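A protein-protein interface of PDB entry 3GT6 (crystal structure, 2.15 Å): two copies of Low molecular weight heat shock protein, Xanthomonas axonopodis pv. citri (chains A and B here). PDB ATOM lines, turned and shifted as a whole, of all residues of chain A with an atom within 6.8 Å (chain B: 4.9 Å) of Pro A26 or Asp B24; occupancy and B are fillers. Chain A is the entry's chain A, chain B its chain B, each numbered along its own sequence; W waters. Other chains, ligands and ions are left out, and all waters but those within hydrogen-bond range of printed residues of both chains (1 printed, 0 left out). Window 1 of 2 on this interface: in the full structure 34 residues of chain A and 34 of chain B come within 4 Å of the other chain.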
ATOM      1  N   TRP A   6       5.653   6.182 -14.966  1.00  0.00           N
ATOM      2  CA  TRP A   6       6.746   6.365 -15.927  1.00  0.00           C
ATOM      3  C   TRP A   6       6.560   5.440 -17.118  1.00  0.00           C
ATOM      4  O   TRP A   6       5.845   4.459 -17.045  1.00  0.00           O
ATOM      5  CB  TRP A   6       8.151   6.183 -15.379  1.00  0.00           C
ATOM      6  CG  TRP A   6       8.651   4.816 -15.117  1.00  0.00           C
ATOM      7  CD1 TRP A   6       8.148   3.949 -14.205  1.00  0.00           C
ATOM      8  CD2 TRP A   6       9.848   4.202 -15.617  1.00  0.00           C
ATOM      9  NE1 TRP A   6       8.927   2.803 -14.126  1.00  0.00           N
ATOM     10  CE2 TRP A   6       9.984   2.935 -14.970  1.00  0.00           C
ATOM     11  CE3 TRP A   6      10.822   4.587 -16.523  1.00  0.00           C
ATOM     12  CZ2 TRP A   6      11.036   2.024 -15.241  1.00  0.00           C
ATOM     13  CZ3 TRP A   6      11.834   3.664 -16.805  1.00  0.00           C
ATOM     14  CH2 TRP A   6      11.946   2.413 -16.149  1.00  0.00           C
ATOM     15  N   PRO A   8       8.694   3.502 -19.670  1.00  0.00           N
ATOM     16  CA  PRO A   8       9.943   2.920 -20.111  1.00  0.00           C
ATOM     17  C   PRO A   8      10.002   2.976 -21.644  1.00  0.00           C
ATOM     18  O   PRO A   8       8.963   2.802 -22.338  1.00  0.00           O
ATOM     19  CB  PRO A   8       9.812   1.461 -19.661  1.00  0.00           C
ATOM     20  CG  PRO A   8       8.848   1.514 -18.466  1.00  0.00           C
ATOM     21  CD  PRO A   8       7.941   2.656 -18.737  1.00  0.00           C
ATOM     22  N   ALA A  23      12.874  -3.431 -24.088  1.00  0.00           N
ATOM     23  CA  ALA A  23      12.324  -2.467 -23.165  1.00  0.00           C
ATOM     24  C   ALA A  23      13.443  -2.114 -22.202  1.00  0.00           C
ATOM     25  O   ALA A  23      14.079  -3.006 -21.604  1.00  0.00           O
ATOM     26  CB  ALA A  23      11.174  -3.089 -22.411  1.00  0.00           C
ATOM     27  N   ASP A  24      13.717  -0.827 -22.048  1.00  0.00           N
ATOM     28  CA  ASP A  24      14.729  -0.383 -21.090  1.00  0.00           C
ATOM     29  C   ASP A  24      14.001  -0.304 -19.788  1.00  0.00           C
ATOM     30  O   ASP A  24      13.204   0.636 -19.536  1.00  0.00           O
ATOM     31  CB  ASP A  24      15.215   1.030 -21.454  1.00  0.00           C
ATOM     32  CG  ASP A  24      16.254   1.016 -22.578  1.00  0.00           C
ATOM     33  OD1 ASP A  24      16.711  -0.043 -22.988  1.00  0.00           O
ATOM     34  OD2 ASP A  24      16.672   2.069 -23.014  1.00  0.00           O
ATOM     35  N   LEU A  25      14.326  -1.267 -18.945  1.00  0.00           N
ATOM     36  CA  LEU A  25      13.674  -1.424 -17.643  1.00  0.00           C
ATOM     37  C   LEU A  25      14.810  -1.544 -16.644  1.00  0.00           C
ATOM     38  O   LEU A  25      14.926  -2.552 -15.956  1.00  0.00           O
ATOM     39  CB  LEU A  25      12.798  -2.691 -17.648  1.00  0.00           C
ATOM     40  CG  LEU A  25      11.579  -2.506 -18.572  1.00  0.00           C
ATOM     41  CD1 LEU A  25      10.732  -3.747 -18.722  1.00  0.00           C
ATOM     42  CD2 LEU A  25      10.745  -1.388 -18.017  1.00  0.00           C
ATOM     43  N   PRO A  26      15.649  -0.495 -16.547  1.00  0.00           N
ATOM     44  CA  PRO A  26      16.757  -0.654 -15.630  1.00  0.00           C
ATOM     45  C   PRO A  26      16.273  -0.785 -14.157  1.00  0.00           C
ATOM     46  O   PRO A  26      15.289  -0.181 -13.764  1.00  0.00           O
ATOM     47  CB  PRO A  26      17.534   0.659 -15.783  1.00  0.00           C
ATOM     48  CG  PRO A  26      16.505   1.687 -16.396  1.00  0.00           C
ATOM     49  CD  PRO A  26      15.672   0.797 -17.285  1.00  0.00           C
ATOM     50  N   GLY A  27      16.997  -1.540 -13.358  1.00  0.00           N
ATOM     51  CA  GLY A  27      16.776  -1.571 -11.904  1.00  0.00           C
ATOM     52  C   GLY A  27      15.585  -2.408 -11.489  1.00  0.00           C
ATOM     53  O   GLY A  27      15.029  -2.141 -10.442  1.00  0.00           O
ATOM     54  N   ILE A  28      15.148  -3.368 -12.317  1.00  0.00           N
ATOM     55  CA  ILE A  28      14.038  -4.280 -11.934  1.00  0.00           C
ATOM     56  C   ILE A  28      14.498  -5.633 -12.327  1.00  0.00           C
ATOM     57  O   ILE A  28      15.051  -5.780 -13.423  1.00  0.00           O
ATOM     58  CB  ILE A  28      12.717  -4.050 -12.745  1.00  0.00           C
ATOM     59  CG1 ILE A  28      12.418  -2.598 -12.896  1.00  0.00           C
ATOM     60  CG2 ILE A  28      11.521  -4.649 -12.052  1.00  0.00           C
ATOM     61  CD1 ILE A  28      11.515  -2.341 -14.054  1.00  0.00           C
ATOM     62  N   ASP A  29      14.276  -6.649 -11.480  1.00  0.00           N
ATOM     63  CA  ASP A  29      14.579  -8.013 -11.914  1.00  0.00           C
ATOM     64  C   ASP A  29      13.591  -8.326 -12.999  1.00  0.00           C
ATOM     65  O   ASP A  29      12.444  -7.975 -12.863  1.00  0.00           O
ATOM     66  CB  ASP A  29      14.338  -9.065 -10.820  1.00  0.00           C
ATOM     67  CG  ASP A  29      15.291  -8.940  -9.695  1.00  0.00           C
ATOM     68  OD1 ASP A  29      16.493  -8.686  -9.964  1.00  0.00           O
ATOM     69  OD2 ASP A  29      14.803  -9.080  -8.540  1.00  0.00           O
ATOM     70  N   ARG A  48       8.906  -0.271 -10.791  1.00  0.00           N
ATOM     71  CA  ARG A  48      10.299  -0.090 -10.476  1.00  0.00           C
ATOM     72  C   ARG A  48      10.349   0.668  -9.179  1.00  0.00           C
ATOM     73  O   ARG A  48       9.672   1.650  -9.016  1.00  0.00           O
ATOM     74  CB  ARG A  48      11.019   0.686 -11.597  1.00  0.00           C
ATOM     75  CG  ARG A  48      12.467   0.829 -11.323  1.00  0.00           C
ATOM     76  CD  ARG A  48      13.039   2.003 -12.151  1.00  0.00           C
ATOM     77  NE  ARG A  48      14.465   2.050 -11.880  1.00  0.00           N
ATOM     78  CZ  ARG A  48      15.346   2.792 -12.522  1.00  0.00           C
ATOM     79  NH1 ARG A  48      14.933   3.643 -13.456  1.00  0.00           N
ATOM     80  NH2 ARG A  48      16.640   2.664 -12.210  1.00  0.00           N
ATOM     81  N   LYS A  49      11.148   0.186  -8.270  1.00  0.00           N
ATOM     82  CA  LYS A  49      11.460   0.908  -7.072  1.00  0.00           C
ATOM     83  C   LYS A  49      12.755   1.671  -7.347  1.00  0.00           C
ATOM     84  O   LYS A  49      13.568   1.315  -8.251  1.00  0.00           O
ATOM     85  CB  LYS A  49      11.775  -0.085  -5.943  1.00  0.00           C
ATOM     86  CG  LYS A  49      10.721  -1.156  -5.666  1.00  0.00           C
ATOM     87  CD  LYS A  49       9.451  -0.476  -5.283  1.00  0.00           C
ATOM     88  CE  LYS A  49       8.324  -1.446  -5.494  1.00  0.00           C
ATOM     89  NZ  LYS A  49       7.450  -1.372  -4.304  1.00  0.00           N
ATOM     90  N   GLU A  63      16.954  11.962 -11.064  1.00  0.00           N
ATOM     91  CA  GLU A  63      16.551  12.046 -12.467  1.00  0.00           C
ATOM     92  C   GLU A  63      15.894  10.754 -12.902  1.00  0.00           C
ATOM     93  O   GLU A  63      15.214  10.719 -13.929  1.00  0.00           O
ATOM     94  CB  GLU A  63      17.758  12.292 -13.380  1.00  0.00           C
ATOM     95  CG  GLU A  63      18.510  13.619 -13.146  1.00  0.00           C
ATOM     96  CD  GLU A  63      19.836  13.631 -13.923  1.00  0.00           C
ATOM     97  OE1 GLU A  63      20.139  12.588 -14.545  1.00  0.00           O
ATOM     98  OE2 GLU A  63      20.576  14.658 -13.938  1.00  0.00           O
ATOM     99  N   ARG A  64      16.141   9.695 -12.156  1.00  0.00           N
ATOM    100  CA  ARG A  64      15.689   8.387 -12.563  1.00  0.00           C
ATOM    101  C   ARG A  64      14.242   8.218 -12.256  1.00  0.00           C
ATOM    102  O   ARG A  64      13.788   8.444 -11.116  1.00  0.00           O
ATOM    103  CB  ARG A  64      16.471   7.325 -11.858  1.00  0.00           C
ATOM    104  CG  ARG A  64      17.972   7.289 -12.364  1.00  0.00           C
ATOM    105  CD  ARG A  64      18.797   6.746 -11.280  1.00  0.00           C
ATOM    106  NE  ARG A  64      18.710   5.317 -11.110  1.00  0.00           N
ATOM    107  CZ  ARG A  64      18.448   4.666  -9.977  1.00  0.00           C
ATOM    108  NH1 ARG A  64      18.188   5.272  -8.833  1.00  0.00           N
ATOM    109  NH2 ARG A  64      18.453   3.344 -10.000  1.00  0.00           N
ATOM    110  N   ARG A  65      13.515   7.831 -13.280  1.00  0.00           N
ATOM    111  CA  ARG A  65      12.094   7.629 -13.175  1.00  0.00           C
ATOM    112  C   ARG A  65      11.831   6.236 -12.663  1.00  0.00           C
ATOM    113  O   ARG A  65      12.567   5.324 -12.938  1.00  0.00           O
ATOM    114  CB  ARG A  65      11.469   7.852 -14.549  1.00  0.00           C
ATOM    115  CG  ARG A  65      11.766   9.321 -15.061  1.00  0.00           C
ATOM    116  CD  ARG A  65      11.023   9.494 -16.393  1.00  0.00           C
ATOM    117  NE  ARG A  65      10.876  10.873 -16.880  1.00  0.00           N
ATOM    118  CZ  ARG A  65      11.127  11.244 -18.133  1.00  0.00           C
ATOM    119  NH1 ARG A  65      11.580  10.369 -19.034  1.00  0.00           N
ATOM    120  NH2 ARG A  65      10.933  12.498 -18.491  1.00  0.00           N
ATOM    121  N   ASN A  90      21.123  -6.768 -18.199  1.00  0.00           N
ATOM    122  CA  ASN A  90      21.495  -5.411 -17.906  1.00  0.00           C
ATOM    123  C   ASN A  90      20.325  -4.405 -18.026  1.00  0.00           C
ATOM    124  O   ASN A  90      20.482  -3.321 -18.589  1.00  0.00           O
ATOM    125  CB  ASN A  90      22.551  -4.985 -18.898  1.00  0.00           C
ATOM    126  CG  ASN A  90      23.835  -5.735 -18.736  1.00  0.00           C
ATOM    127  OD1 ASN A  90      24.459  -6.132 -19.732  1.00  0.00           O
ATOM    128  ND2 ASN A  90      24.232  -5.960 -17.507  1.00  0.00           N
ATOM    129  N   GLY A  91      19.153  -4.762 -17.543  1.00  0.00           N
ATOM    130  CA  GLY A  91      18.125  -3.778 -17.482  1.00  0.00           C
ATOM    131  C   GLY A  91      17.343  -3.732 -18.770  1.00  0.00           C
ATOM    132  O   GLY A  91      16.374  -3.046 -18.806  1.00  0.00           O
ATOM    133  N   VAL A  92      17.733  -4.464 -19.814  1.00  0.00           N
ATOM    134  CA  VAL A  92      16.959  -4.419 -21.064  1.00  0.00           C
ATOM    135  C   VAL A  92      16.149  -5.714 -21.139  1.00  0.00           C
ATOM    136  O   VAL A  92      16.707  -6.770 -21.059  1.00  0.00           O
ATOM    137  CB  VAL A  92      17.858  -4.291 -22.275  1.00  0.00           C
ATOM    138  CG1 VAL A  92      17.036  -4.465 -23.525  1.00  0.00           C
ATOM    139  CG2 VAL A  92      18.492  -2.862 -22.360  1.00  0.00           C
ATOM    140  N   TRP B   6      22.384  10.122 -26.091  1.00  0.00           N
ATOM    141  CA  TRP B   6      21.911   9.438 -24.914  1.00  0.00           C
ATOM    142  C   TRP B   6      22.417  10.230 -23.667  1.00  0.00           C
ATOM    143  O   TRP B   6      23.598  10.504 -23.545  1.00  0.00           O
ATOM    144  CB  TRP B   6      22.426   8.026 -24.915  1.00  0.00           C
ATOM    145  CG  TRP B   6      21.927   7.241 -23.828  1.00  0.00           C
ATOM    146  CD1 TRP B   6      20.779   7.454 -23.093  1.00  0.00           C
ATOM    147  CD2 TRP B   6      22.494   6.059 -23.340  1.00  0.00           C
ATOM    148  NE1 TRP B   6      20.620   6.463 -22.168  1.00  0.00           N
ATOM    149  CE2 TRP B   6      21.664   5.588 -22.306  1.00  0.00           C
ATOM    150  CE3 TRP B   6      23.640   5.356 -23.649  1.00  0.00           C
ATOM    151  CZ2 TRP B   6      21.931   4.457 -21.628  1.00  0.00           C
ATOM    152  CZ3 TRP B   6      23.908   4.218 -22.954  1.00  0.00           C
ATOM    153  CH2 TRP B   6      23.050   3.764 -21.971  1.00  0.00           C
ATOM    154  N   PRO B   8      22.102   9.338 -19.913  1.00  0.00           N
ATOM    155  CA  PRO B   8      21.514   8.361 -19.003  1.00  0.00           C
ATOM    156  C   PRO B   8      21.207   9.077 -17.697  1.00  0.00           C
ATOM    157  O   PRO B   8      22.021   9.896 -17.209  1.00  0.00           O
ATOM    158  CB  PRO B   8      22.639   7.355 -18.746  1.00  0.00           C
ATOM    159  CG  PRO B   8      23.702   7.680 -19.757  1.00  0.00           C
ATOM    160  CD  PRO B   8      23.444   8.984 -20.385  1.00  0.00           C
ATOM    161  N   ARG B   9      20.074   8.757 -17.124  1.00  0.00           N
ATOM    162  CA  ARG B   9      19.588   9.435 -15.906  1.00  0.00           C
ATOM    163  C   ARG B   9      20.328   8.897 -14.710  1.00  0.00           C
ATOM    164  O   ARG B   9      20.625   7.715 -14.635  1.00  0.00           O
ATOM    165  CB  ARG B   9      18.080   9.221 -15.775  1.00  0.00           C
ATOM    166  CG  ARG B   9      17.358  10.113 -16.820  1.00  0.00           C
ATOM    167  CD  ARG B   9      15.863   9.707 -16.891  1.00  0.00           C
ATOM    168  NE  ARG B   9      15.246  10.649 -17.834  1.00  0.00           N
ATOM    169  CZ  ARG B   9      14.750  11.825 -17.495  1.00  0.00           C
ATOM    170  NH1 ARG B   9      14.688  12.210 -16.220  1.00  0.00           N
ATOM    171  NH2 ARG B   9      14.265  12.622 -18.444  1.00  0.00           N
ATOM    172  N   TYR B  22      23.592   6.664  -8.816  1.00  0.00           N
ATOM    173  CA  TYR B  22      22.931   5.525  -9.399  1.00  0.00           C
ATOM    174  C   TYR B  22      22.687   5.994 -10.813  1.00  0.00           C
ATOM    175  O   TYR B  22      22.143   7.051 -10.999  1.00  0.00           O
ATOM    176  CB  TYR B  22      21.549   5.324  -8.791  1.00  0.00           C
ATOM    177  CG  TYR B  22      21.592   5.137  -7.284  1.00  0.00           C
ATOM    178  CD1 TYR B  22      21.736   3.875  -6.723  1.00  0.00           C
ATOM    179  CD2 TYR B  22      21.514   6.223  -6.446  1.00  0.00           C
ATOM    180  CE1 TYR B  22      21.817   3.715  -5.358  1.00  0.00           C
ATOM    181  CE2 TYR B  22      21.542   6.073  -5.126  1.00  0.00           C
ATOM    182  CZ  TYR B  22      21.680   4.830  -4.576  1.00  0.00           C
ATOM    183  OH  TYR B  22      21.718   4.738  -3.200  1.00  0.00           O
ATOM    184  N   ALA B  23      23.022   5.166 -11.788  1.00  0.00           N
ATOM    185  CA  ALA B  23      22.939   5.580 -13.180  1.00  0.00           C
ATOM    186  C   ALA B  23      22.195   4.506 -13.921  1.00  0.00           C
ATOM    187  O   ALA B  23      22.541   3.302 -13.887  1.00  0.00           O
ATOM    188  CB  ALA B  23      24.309   5.751 -13.742  1.00  0.00           C
ATOM    189  N   ASP B  24      21.132   4.906 -14.557  1.00  0.00           N
ATOM    190  CA  ASP B  24      20.418   3.983 -15.390  1.00  0.00           C
ATOM    191  C   ASP B  24      21.194   3.845 -16.714  1.00  0.00           C
ATOM    192  O   ASP B  24      21.071   4.694 -17.606  1.00  0.00           O
ATOM    193  CB  ASP B  24      19.042   4.548 -15.693  1.00  0.00           C
ATOM    194  CG  ASP B  24      18.094   4.339 -14.528  1.00  0.00           C
ATOM    195  OD1 ASP B  24      18.484   3.694 -13.569  1.00  0.00           O
ATOM    196  OD2 ASP B  24      16.979   4.803 -14.556  1.00  0.00           O
ATOM    197  N   LEU B  25      21.869   2.711 -16.852  1.00  0.00           N
ATOM    198  CA  LEU B  25      22.691   2.408 -18.018  1.00  0.00           C
ATOM    199  C   LEU B  25      22.230   1.081 -18.560  1.00  0.00           C
ATOM    200  O   LEU B  25      23.022   0.162 -18.690  1.00  0.00           O
ATOM    201  CB  LEU B  25      24.168   2.367 -17.604  1.00  0.00           C
ATOM    202  CG  LEU B  25      24.566   3.820 -17.203  1.00  0.00           C
ATOM    203  CD1 LEU B  25      25.969   3.924 -16.615  1.00  0.00           C
ATOM    204  CD2 LEU B  25      24.523   4.648 -18.424  1.00  0.00           C
ATOM    205  N   PRO B  26      20.950   0.995 -18.919  1.00  0.00           N
ATOM    206  CA  PRO B  26      20.497  -0.282 -19.421  1.00  0.00           C
ATOM    207  C   PRO B  26      21.221  -0.696 -20.731  1.00  0.00           C
ATOM    208  O   PRO B  26      21.501   0.150 -21.609  1.00  0.00           O
ATOM    209  CB  PRO B  26      19.036  -0.024 -19.703  1.00  0.00           C
ATOM    210  CG  PRO B  26      18.951   1.491 -19.951  1.00  0.00           C
ATOM    211  CD  PRO B  26      19.914   2.034 -18.950  1.00  0.00           C
ATOM    212  N   ASN B  90      21.025  -5.178 -13.285  1.00  0.00           N
ATOM    213  CA  ASN B  90      19.842  -4.831 -14.025  1.00  0.00           C
ATOM    214  C   ASN B  90      20.005  -3.478 -14.707  1.00  0.00           C
ATOM    215  O   ASN B  90      19.072  -2.697 -14.728  1.00  0.00           O
ATOM    216  CB  ASN B  90      18.700  -4.796 -13.043  1.00  0.00           C
ATOM    217  CG  ASN B  90      18.318  -6.173 -12.616  1.00  0.00           C
ATOM    218  OD1 ASN B  90      18.010  -6.408 -11.457  1.00  0.00           O
ATOM    219  ND2 ASN B  90      18.440  -7.104 -13.517  1.00  0.00           N
ATOM    220  N   GLY B  91      21.227  -3.173 -15.123  1.00  0.00           N
ATOM    221  CA  GLY B  91      21.526  -1.951 -15.897  1.00  0.00           C
ATOM    222  C   GLY B  91      21.583  -0.690 -15.080  1.00  0.00           C
ATOM    223  O   GLY B  91      21.536   0.413 -15.645  1.00  0.00           O
ATOM    224  N   VAL B  92      21.584  -0.815 -13.747  1.00  0.00           N
ATOM    225  CA  VAL B  92      21.811   0.390 -12.884  1.00  0.00           C
ATOM    226  C   VAL B  92      23.249   0.302 -12.478  1.00  0.00           C
ATOM    227  O   VAL B  92      23.691  -0.711 -12.027  1.00  0.00           O
ATOM    228  CB  VAL B  92      20.907   0.466 -11.625  1.00  0.00           C
ATOM    229  CG1 VAL B  92      21.316   1.623 -10.712  1.00  0.00           C
ATOM    230  CG2 VAL B  92      19.420   0.574 -11.986  1.00  0.00           C
HETATM  231  O   HOH W   1      17.693  -4.126  -9.697  1.00  0.00           O
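Among the printed residues, merely in contact across the chains: Asp A24 with Pro B26 (3.8 Å), Pro A26 with Asp B24 (3.6 Å), Pro A26 with Asn B90 (3.2 Å), Gly A27 with Val B92 (3.4 Å), Ile A28 with Asn B90 (3.4 Å), Arg A48 with Val B92 (3.5 Å), Arg A64 with Arg B9 (3.5 Å), Arg A64 with Tyr B22 (3.4 Å), Arg A64 with Val B92 (3.4 Å), Asn A90 with Pro B26 (3.2 Å), Asn A90 with Asn B90 (3.5 Å), Asn A90 with Gly B91 (3.2 Å), Gly A91 with Gly B91 (3.6 Å) and Val A92 with Pro B26 (3.8 Å).
Water W1 bridges the side-chain amide oxygen (OD1) of Asn B90 and the backbone carbonyl oxygen (O) of Gly A27.
Pro A26 touches Asn B90, and with the chains exchanged Asn A90 touches Pro B26.
Asn A90 touches Gly B91, and with the chains exchanged Gly A91 touches Asn B90.
Gly B91 touches its own counterpart, Gly A91.
Val A92 touches Pro B26, but with the chains exchanged Pro A26 does not touch Val B92 (4.1 Å).
Of the 21 pairs that touch across the chains among the printed residues, 8 have their exchanged pair printed and touching as well.
Printed residues of chain B within 4 Å of Pro A26: Asp B24 and Asn B90.
Printed residues of chain B within 4 Å of Ile A28: Asn B90.
Printed residues of chain B within 4 Å of Asp A29: Asn B90 (3.1 Å).
Printed residues of chain B within 4 Å of Arg A48: Asp B24 (2.5 Å) and Val B92 (3.5 Å).
Printed residues of chain B within 4 Å of Gly A91: Asn B90 (3.1 Å) and Gly B91 (3.6 Å).
Ala B23 touches none of the printed residues of chain A.
Leu B25 touches none of the printed residues of chain A.
Printed residues of chain A within 4 Å of Val B92: Gly A27 (3.4 Å), Arg A48 (3.5 Å) and Arg A64 (3.4 Å).
The nearest printed residue of chain A that does not touch Asp B24 is Arg A65 (4.7 Å).
The nearest printed residue of chain B that does not touch Gly A91 is Pro B26 (4.1 Å).
Printed residues of chain B that touch a printed residue of chain A: Arg B9, Tyr B22, Asp B24, Pro B26, Asn B90, Gly B91 and Val B92.
Hydrophobic or aromatic side chains of chain B within 4 Å of the printed part of chain A: Tyr B22, Pro B26 and Val B92.
Along chain B the printed residues that touch a printed residue of chain A span positions 9 to 92.
Hydrophobic or aromatic side chains of chain A that line the printed part of chain B: Pro A26 and Val A92.
Along chain A the printed residues that touch a printed residue of chain B span positions 24 to 92.
Among the printed residues, Asp or Glu carboxylates within 4 Å of a Lys or Arg side-chain nitrogen of the other chain: Arg A48 with Asp B24 (2.5 Å) and Arg A64 with Asp B24 (3.0 Å).
The backbone NH of Gly A27 lies within hydrogen-bond range of the backbone carbonyl oxygen of Asn B90.
The side-chain carboxylate (OD1) of Asp A29 sits close to the side-chain amide oxygen (OD1) of Asn B90, at 3.1 Å.
The side-chain carboxylate of Asp B24 lies within salt-bridge range of the guanidinium group of Arg A48 (2.5 Å).
The backbone carbonyl oxygen (O) of Glu A63 lies within hydrogen-bond range of the guanidinium group (NH1) of Arg B9 (2.8 Å).
The guanidinium group of Arg A64 lies within salt-bridge range of the side-chain carboxylate of Asp B24, at 3.0 Å.
The backbone NH (N) of Gly A91 lies close to the backbone carbonyl oxygen (O) of Asn B90, at 3.5 Å.
The guanidinium group (NH2) of Arg B9 lies close to the guanidinium group (NH2) of Arg A65, at 3.3 Å.
N of Leu A25 lies within hydrogen-bond range of O of Gly A91, at 2.7 Å.
The backbone carbonyl oxygen (O) of Pro A26 is in hydrogen-bond range of the guanidinium group (NE) of Arg A48 (3.0 Å).
The guanidinium group (NH1) of Arg A48 sits at hydrogen-bond distance from the backbone carbonyl oxygen (O) of Arg A65, 2.9 Å away.
The backbone carbonyl oxygen of Arg B9 is in hydrogen-bond range of the backbone NH of Asp B24.
The backbone carbonyl oxygen (O) of Gly B91 lies within hydrogen-bond range of the backbone NH (N) of Leu B25 (2.6 Å).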
